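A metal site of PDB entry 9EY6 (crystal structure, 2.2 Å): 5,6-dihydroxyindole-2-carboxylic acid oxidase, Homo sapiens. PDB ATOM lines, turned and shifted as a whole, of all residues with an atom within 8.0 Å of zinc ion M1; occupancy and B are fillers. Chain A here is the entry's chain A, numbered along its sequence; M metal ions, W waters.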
ATOM      1  N   HIS A 168      18.030  29.493  13.415  1.00  0.00           N
ATOM      2  CA  HIS A 168      17.918  28.040  13.516  1.00  0.00           C
ATOM      3  C   HIS A 168      19.246  27.440  14.014  1.00  0.00           C
ATOM      4  O   HIS A 168      19.231  26.572  14.884  1.00  0.00           O
ATOM      5  CB  HIS A 168      17.467  27.421  12.181  1.00  0.00           C
ATOM      6  CG  HIS A 168      17.038  25.966  12.189  1.00  0.00           C
ATOM      7  ND1 HIS A 168      17.919  24.926  12.004  1.00  0.00           N
ATOM      8  CD2 HIS A 168      15.811  25.372  12.300  1.00  0.00           C
ATOM      9  CE1 HIS A 168      17.243  23.767  11.965  1.00  0.00           C
ATOM     10  NE2 HIS A 168      15.948  23.994  12.199  1.00  0.00           N
ATOM     11  N   TYR A 169      20.370  27.913  13.491  1.00  0.00           N
ATOM     12  CA  TYR A 169      21.692  27.482  13.920  1.00  0.00           C
ATOM     13  C   TYR A 169      21.887  27.740  15.419  1.00  0.00           C
ATOM     14  O   TYR A 169      22.289  26.837  16.152  1.00  0.00           O
ATOM     15  CB  TYR A 169      22.778  28.198  13.090  1.00  0.00           C
ATOM     16  CG  TYR A 169      24.080  28.421  13.850  1.00  0.00           C
ATOM     17  CD1 TYR A 169      25.035  27.423  14.002  1.00  0.00           C
ATOM     18  CD2 TYR A 169      24.338  29.647  14.424  1.00  0.00           C
ATOM     19  CE1 TYR A 169      26.191  27.623  14.750  1.00  0.00           C
ATOM     20  CE2 TYR A 169      25.464  29.867  15.194  1.00  0.00           C
ATOM     21  CZ  TYR A 169      26.400  28.860  15.359  1.00  0.00           C
ATOM     22  OH  TYR A 169      27.501  29.210  16.100  1.00  0.00           O
ATOM     23  N   SER A 171      19.800  28.108  17.765  1.00  0.00           N
ATOM     24  CA  SER A 171      18.957  27.255  18.591  1.00  0.00           C
ATOM     25  C   SER A 171      19.475  25.829  18.780  1.00  0.00           C
ATOM     26  O   SER A 171      18.988  25.135  19.694  1.00  0.00           O
ATOM     27  CB  SER A 171      17.526  27.245  18.061  1.00  0.00           C
ATOM     28  OG  SER A 171      17.350  26.432  16.916  1.00  0.00           O
ATOM     29  N   VAL A 172      20.402  25.348  17.918  1.00  0.00           N
ATOM     30  CA  VAL A 172      20.867  23.965  17.951  1.00  0.00           C
ATOM     31  C   VAL A 172      22.352  23.865  18.291  1.00  0.00           C
ATOM     32  O   VAL A 172      22.859  22.774  18.470  1.00  0.00           O
ATOM     33  CB  VAL A 172      20.566  23.130  16.672  1.00  0.00           C
ATOM     34  CG1 VAL A 172      19.100  23.140  16.280  1.00  0.00           C
ATOM     35  CG2 VAL A 172      21.419  23.531  15.476  1.00  0.00           C
ATOM     36  N   ASP A 188      18.999  21.110  22.549  1.00  0.00           N
ATOM     37  CA  ASP A 188      18.412  21.578  21.308  1.00  0.00           C
ATOM     38  C   ASP A 188      17.147  22.372  21.644  1.00  0.00           C
ATOM     39  O   ASP A 188      16.141  21.782  22.030  1.00  0.00           O
ATOM     40  CB  ASP A 188      18.122  20.397  20.396  1.00  0.00           C
ATOM     41  CG  ASP A 188      17.803  20.717  18.931  1.00  0.00           C
ATOM     42  OD1 ASP A 188      17.045  21.704  18.689  1.00  0.00           O
ATOM     43  OD2 ASP A 188      18.286  19.955  18.028  1.00  0.00           O
ATOM     44  N   SER A 190      14.947  23.745  19.747  1.00  0.00           N
ATOM     45  CA  SER A 190      13.949  23.821  18.678  1.00  0.00           C
ATOM     46  C   SER A 190      13.576  22.445  18.127  1.00  0.00           C
ATOM     47  O   SER A 190      12.670  22.353  17.312  1.00  0.00           O
ATOM     48  CB  SER A 190      14.417  24.683  17.584  1.00  0.00           C
ATOM     49  OG  SER A 190      15.774  24.391  17.224  1.00  0.00           O
ATOM     50  N   HIS A 191      14.248  21.371  18.568  1.00  0.00           N
ATOM     51  CA  HIS A 191      13.927  20.018  18.135  1.00  0.00           C
ATOM     52  C   HIS A 191      13.968  19.089  19.350  1.00  0.00           C
ATOM     53  O   HIS A 191      14.544  19.443  20.386  1.00  0.00           O
ATOM     54  CB  HIS A 191      14.950  19.534  17.091  1.00  0.00           C
ATOM     55  CG  HIS A 191      15.212  20.507  15.974  1.00  0.00           C
ATOM     56  ND1 HIS A 191      16.076  21.570  16.116  1.00  0.00           N
ATOM     57  CD2 HIS A 191      14.682  20.619  14.757  1.00  0.00           C
ATOM     58  CE1 HIS A 191      16.048  22.292  15.010  1.00  0.00           C
ATOM     59  NE2 HIS A 191      15.236  21.703  14.156  1.00  0.00           N
ATOM     60  N   PHE A 196       9.196  21.907  19.276  1.00  0.00           N
ATOM     61  CA  PHE A 196       9.505  21.721  17.856  1.00  0.00           C
ATOM     62  C   PHE A 196       8.554  22.508  16.923  1.00  0.00           C
ATOM     63  O   PHE A 196       9.019  23.327  16.109  1.00  0.00           O
ATOM     64  CB  PHE A 196       9.535  20.242  17.491  1.00  0.00           C
ATOM     65  CG  PHE A 196       9.560  19.947  16.004  1.00  0.00           C
ATOM     66  CD1 PHE A 196      10.649  20.288  15.231  1.00  0.00           C
ATOM     67  CD2 PHE A 196       8.465  19.391  15.384  1.00  0.00           C
ATOM     68  CE1 PHE A 196      10.638  20.048  13.871  1.00  0.00           C
ATOM     69  CE2 PHE A 196       8.462  19.153  14.030  1.00  0.00           C
ATOM     70  CZ  PHE A 196       9.550  19.473  13.266  1.00  0.00           C
ATOM     71  N   TRP A 199       8.146  26.481  17.761  1.00  0.00           N
ATOM     72  CA  TRP A 199       9.373  27.164  17.341  1.00  0.00           C
ATOM     73  C   TRP A 199       9.381  27.382  15.825  1.00  0.00           C
ATOM     74  O   TRP A 199       9.567  28.506  15.342  1.00  0.00           O
ATOM     75  CB  TRP A 199      10.622  26.420  17.825  1.00  0.00           C
ATOM     76  CG  TRP A 199      11.908  27.202  17.705  1.00  0.00           C
ATOM     77  CD1 TRP A 199      12.557  27.816  18.722  1.00  0.00           C
ATOM     78  CD2 TRP A 199      12.692  27.487  16.526  1.00  0.00           C
ATOM     79  NE1 TRP A 199      13.659  28.488  18.254  1.00  0.00           N
ATOM     80  CE2 TRP A 199      13.756  28.310  16.912  1.00  0.00           C
ATOM     81  CE3 TRP A 199      12.562  27.158  15.175  1.00  0.00           C
ATOM     82  CZ2 TRP A 199      14.710  28.783  16.037  1.00  0.00           C
ATOM     83  CZ3 TRP A 199      13.528  27.603  14.291  1.00  0.00           C
ATOM     84  CH2 TRP A 199      14.563  28.412  14.709  1.00  0.00           C
ATOM     85  N   HIS A 200       9.157  26.322  15.047  1.00  0.00           N
ATOM     86  CA  HIS A 200       9.256  26.409  13.588  1.00  0.00           C
ATOM     87  C   HIS A 200       8.119  27.238  13.014  1.00  0.00           C
ATOM     88  O   HIS A 200       8.245  27.854  11.972  1.00  0.00           O
ATOM     89  CB  HIS A 200       9.352  25.000  12.967  1.00  0.00           C
ATOM     90  CG  HIS A 200      10.679  24.332  13.178  1.00  0.00           C
ATOM     91  ND1 HIS A 200      10.999  23.724  14.373  1.00  0.00           N
ATOM     92  CD2 HIS A 200      11.788  24.204  12.375  1.00  0.00           C
ATOM     93  CE1 HIS A 200      12.247  23.235  14.286  1.00  0.00           C
ATOM     94  NE2 HIS A 200      12.756  23.498  13.087  1.00  0.00           N
ATOM     95  N   HIS A 203       9.284  30.861  13.408  1.00  0.00           N
ATOM     96  CA  HIS A 203      10.374  30.997  12.447  1.00  0.00           C
ATOM     97  C   HIS A 203       9.839  31.412  11.072  1.00  0.00           C
ATOM     98  O   HIS A 203      10.353  32.356  10.491  1.00  0.00           O
ATOM     99  CB  HIS A 203      11.063  29.633  12.374  1.00  0.00           C
ATOM    100  CG  HIS A 203      12.371  29.637  11.742  1.00  0.00           C
ATOM    101  ND1 HIS A 203      12.805  28.567  10.969  1.00  0.00           N
ATOM    102  CD2 HIS A 203      13.389  30.523  11.788  1.00  0.00           C
ATOM    103  CE1 HIS A 203      14.044  28.822  10.572  1.00  0.00           C
ATOM    104  NE2 HIS A 203      14.426  30.024  11.042  1.00  0.00           N
ATOM    105  N   GLU A 336       7.216  15.074  14.090  1.00  0.00           N
ATOM    106  CA  GLU A 336       8.624  15.414  13.981  1.00  0.00           C
ATOM    107  C   GLU A 336       9.328  14.280  13.230  1.00  0.00           C
ATOM    108  O   GLU A 336      10.327  14.517  12.537  1.00  0.00           O
ATOM    109  CB  GLU A 336       9.216  15.742  15.353  1.00  0.00           C
ATOM    110  CG  GLU A 336      10.677  16.223  15.317  1.00  0.00           C
ATOM    111  CD  GLU A 336      11.255  16.779  16.629  1.00  0.00           C
ATOM    112  OE1 GLU A 336      10.539  16.729  17.658  1.00  0.00           O
ATOM    113  OE2 GLU A 336      12.441  17.242  16.665  1.00  0.00           O
ATOM    114  N   HIS A 353       8.472  14.545   9.026  1.00  0.00           N
ATOM    115  CA  HIS A 353       9.343  15.697   8.847  1.00  0.00           C
ATOM    116  C   HIS A 353      10.791  15.266   8.696  1.00  0.00           C
ATOM    117  O   HIS A 353      11.501  15.777   7.843  1.00  0.00           O
ATOM    118  CB  HIS A 353       9.058  16.762   9.914  1.00  0.00           C
ATOM    119  CG  HIS A 353      10.256  17.506  10.366  1.00  0.00           C
ATOM    120  ND1 HIS A 353      11.201  17.069  11.275  1.00  0.00           N
ATOM    121  CD2 HIS A 353      10.667  18.720   9.919  1.00  0.00           C
ATOM    122  CE1 HIS A 353      12.163  18.008  11.350  1.00  0.00           C
ATOM    123  NE2 HIS A 353      11.834  19.034  10.536  1.00  0.00           N
ATOM    124  N   ASN A 354      11.253  14.354   9.563  1.00  0.00           N
ATOM    125  CA  ASN A 354      12.661  13.950   9.555  1.00  0.00           C
ATOM    126  C   ASN A 354      12.989  13.185   8.260  1.00  0.00           C
ATOM    127  O   ASN A 354      14.090  13.311   7.749  1.00  0.00           O
ATOM    128  CB  ASN A 354      13.056  13.109  10.757  1.00  0.00           C
ATOM    129  CG  ASN A 354      13.132  13.858  12.076  1.00  0.00           C
ATOM    130  OD1 ASN A 354      13.458  15.056  12.151  1.00  0.00           O
ATOM    131  ND2 ASN A 354      12.862  13.129  13.136  1.00  0.00           N
ATOM    132  N   HIS A 357      13.493  15.678   5.341  1.00  0.00           N
ATOM    133  CA  HIS A 357      14.840  16.221   5.363  1.00  0.00           C
ATOM    134  C   HIS A 357      15.873  15.212   4.862  1.00  0.00           C
ATOM    135  O   HIS A 357      16.799  15.547   4.117  1.00  0.00           O
ATOM    136  CB  HIS A 357      15.230  16.621   6.793  1.00  0.00           C
ATOM    137  CG  HIS A 357      14.783  17.942   7.310  1.00  0.00           C
ATOM    138  ND1 HIS A 357      15.448  19.117   6.991  1.00  0.00           N
ATOM    139  CD2 HIS A 357      13.794  18.299   8.126  1.00  0.00           C
ATOM    140  CE1 HIS A 357      14.871  20.137   7.610  1.00  0.00           C
ATOM    141  NE2 HIS A 357      13.888  19.674   8.322  1.00  0.00           N
ATOM    142  N   GLN A 366      21.367  18.308   7.381  1.00  0.00           N
ATOM    143  CA  GLN A 366      22.256  18.519   8.512  1.00  0.00           C
ATOM    144  C   GLN A 366      21.693  19.654   9.383  1.00  0.00           C
ATOM    145  O   GLN A 366      21.420  20.751   8.884  1.00  0.00           O
ATOM    146  CB  GLN A 366      23.615  18.864   7.902  1.00  0.00           C
ATOM    147  CG  GLN A 366      24.061  17.879   6.821  1.00  0.00           C
ATOM    148  CD  GLN A 366      25.302  18.321   6.096  1.00  0.00           C
ATOM    149  OE1 GLN A 366      26.377  18.495   6.680  1.00  0.00           O
ATOM    150  NE2 GLN A 366      25.177  18.488   4.782  1.00  0.00           N
ATOM    151  N   THR A 367      21.535  19.385  10.682  1.00  0.00           N
ATOM    152  CA  THR A 367      20.614  20.184  11.494  1.00  0.00           C
ATOM    153  C   THR A 367      21.114  21.618  11.628  1.00  0.00           C
ATOM    154  O   THR A 367      20.307  22.550  11.517  1.00  0.00           O
ATOM    155  CB  THR A 367      20.288  19.551  12.846  1.00  0.00           C
ATOM    156  OG1 THR A 367      19.878  18.202  12.600  1.00  0.00           O
ATOM    157  CG2 THR A 367      19.140  20.285  13.526  1.00  0.00           C
ATOM    158  N   HIS A 368      22.446  21.822  11.719  1.00  0.00           N
ATOM    159  CA  HIS A 368      22.967  23.186  11.792  1.00  0.00           C
ATOM    160  C   HIS A 368      22.938  23.964  10.463  1.00  0.00           C
ATOM    161  O   HIS A 368      23.088  25.195  10.497  1.00  0.00           O
ATOM    162  CB  HIS A 368      24.389  23.236  12.357  1.00  0.00           C
ATOM    163  CG  HIS A 368      25.374  22.552  11.481  1.00  0.00           C
ATOM    164  ND1 HIS A 368      25.240  21.205  11.206  1.00  0.00           N
ATOM    165  CD2 HIS A 368      26.436  22.987  10.789  1.00  0.00           C
ATOM    166  CE1 HIS A 368      26.218  20.837  10.375  1.00  0.00           C
ATOM    167  NE2 HIS A 368      26.958  21.900  10.111  1.00  0.00           N
ATOM    168  N   SER A 370      20.388  23.180   7.706  1.00  0.00           N
ATOM    169  CA  SER A 370      19.330  22.771   6.791  1.00  0.00           C
ATOM    170  C   SER A 370      18.579  23.935   6.141  1.00  0.00           C
ATOM    171  O   SER A 370      18.107  23.781   5.023  1.00  0.00           O
ATOM    172  CB  SER A 370      18.362  21.779   7.412  1.00  0.00           C
ATOM    173  OG  SER A 370      18.000  22.150   8.714  1.00  0.00           O
ATOM    174  N   PRO A 371      18.310  25.068   6.826  1.00  0.00           N
ATOM    175  CA  PRO A 371      17.578  26.165   6.190  1.00  0.00           C
ATOM    176  C   PRO A 371      18.313  26.828   5.042  1.00  0.00           C
ATOM    177  O   PRO A 371      17.668  27.540   4.282  1.00  0.00           O
ATOM    178  CB  PRO A 371      17.272  27.162   7.313  1.00  0.00           C
ATOM    179  CG  PRO A 371      17.678  26.468   8.577  1.00  0.00           C
ATOM    180  CD  PRO A 371      18.618  25.352   8.238  1.00  0.00           C
ATOM    181  N   PHE A 376      13.621  23.837   2.732  1.00  0.00           N
ATOM    182  CA  PHE A 376      13.330  23.953   4.150  1.00  0.00           C
ATOM    183  C   PHE A 376      12.057  24.774   4.378  1.00  0.00           C
ATOM    184  O   PHE A 376      11.202  24.349   5.123  1.00  0.00           O
ATOM    185  CB  PHE A 376      14.506  24.589   4.897  1.00  0.00           C
ATOM    186  CG  PHE A 376      14.310  24.703   6.412  1.00  0.00           C
ATOM    187  CD1 PHE A 376      13.553  25.722   6.953  1.00  0.00           C
ATOM    188  CD2 PHE A 376      14.945  23.825   7.282  1.00  0.00           C
ATOM    189  CE1 PHE A 376      13.385  25.821   8.318  1.00  0.00           C
ATOM    190  CE2 PHE A 376      14.781  23.913   8.666  1.00  0.00           C
ATOM    191  CZ  PHE A 376      14.015  24.927   9.185  1.00  0.00           C
ATOM    192  N   HIS A 380       8.745  23.014   5.976  1.00  0.00           N
ATOM    193  CA  HIS A 380       8.244  23.513   7.258  1.00  0.00           C
ATOM    194  C   HIS A 380       6.845  24.120   7.163  1.00  0.00           C
ATOM    195  O   HIS A 380       6.106  24.010   8.136  1.00  0.00           O
ATOM    196  CB  HIS A 380       9.302  24.368   7.996  1.00  0.00           C
ATOM    197  CG  HIS A 380      10.173  23.465   8.795  1.00  0.00           C
ATOM    198  ND1 HIS A 380       9.629  22.916   9.946  1.00  0.00           N
ATOM    199  CD2 HIS A 380      11.386  22.879   8.612  1.00  0.00           C
ATOM    200  CE1 HIS A 380      10.504  22.054  10.449  1.00  0.00           C
ATOM    201  NE2 HIS A 380      11.572  22.015   9.658  1.00  0.00           N
HETATM  202 ZN    ZN M   1      14.550  22.650  12.450  1.00  0.00          ZN
HETATM  203 ZN    ZN M   2      12.963  20.627   9.918  1.00  0.00          ZN
HETATM  204  O   HOH W   1      14.218  21.184  10.797  1.00  0.00           O
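A ring nitrogen (ND1) of His 191 sits at hydrogen-bond distance from the side-chain carboxylate (OD1) of Asp 188 (2.8 Å). ND1 of His 168 sits close to O of Thr 367, 3.4 Å away. The backbone carbonyl oxygen (O) of His 168 is in hydrogen-bond range of the side-chain hydroxyl (OG) of Ser 171, 2.8 Å away. ND1 of His 191 sits at hydrogen-bond distance from OG of Ser 190 (3.0 Å). ND1 of His 200 is in hydrogen-bond range of O of Phe 196 (2.7 Å).
Phe 376 touches zinc ion M1. The nearest printed residue that does not touch zinc ion M1 is His 380 (4.1 Å).
Zinc ion M1 is bound by a ring nitrogen (NE2) of His 168 (2.0 Å), a ring nitrogen (NE2) of His 191 (2.1 Å), a ring nitrogen (NE2) of His 200 (2.1 Å) and water W1 (2.2 Å).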
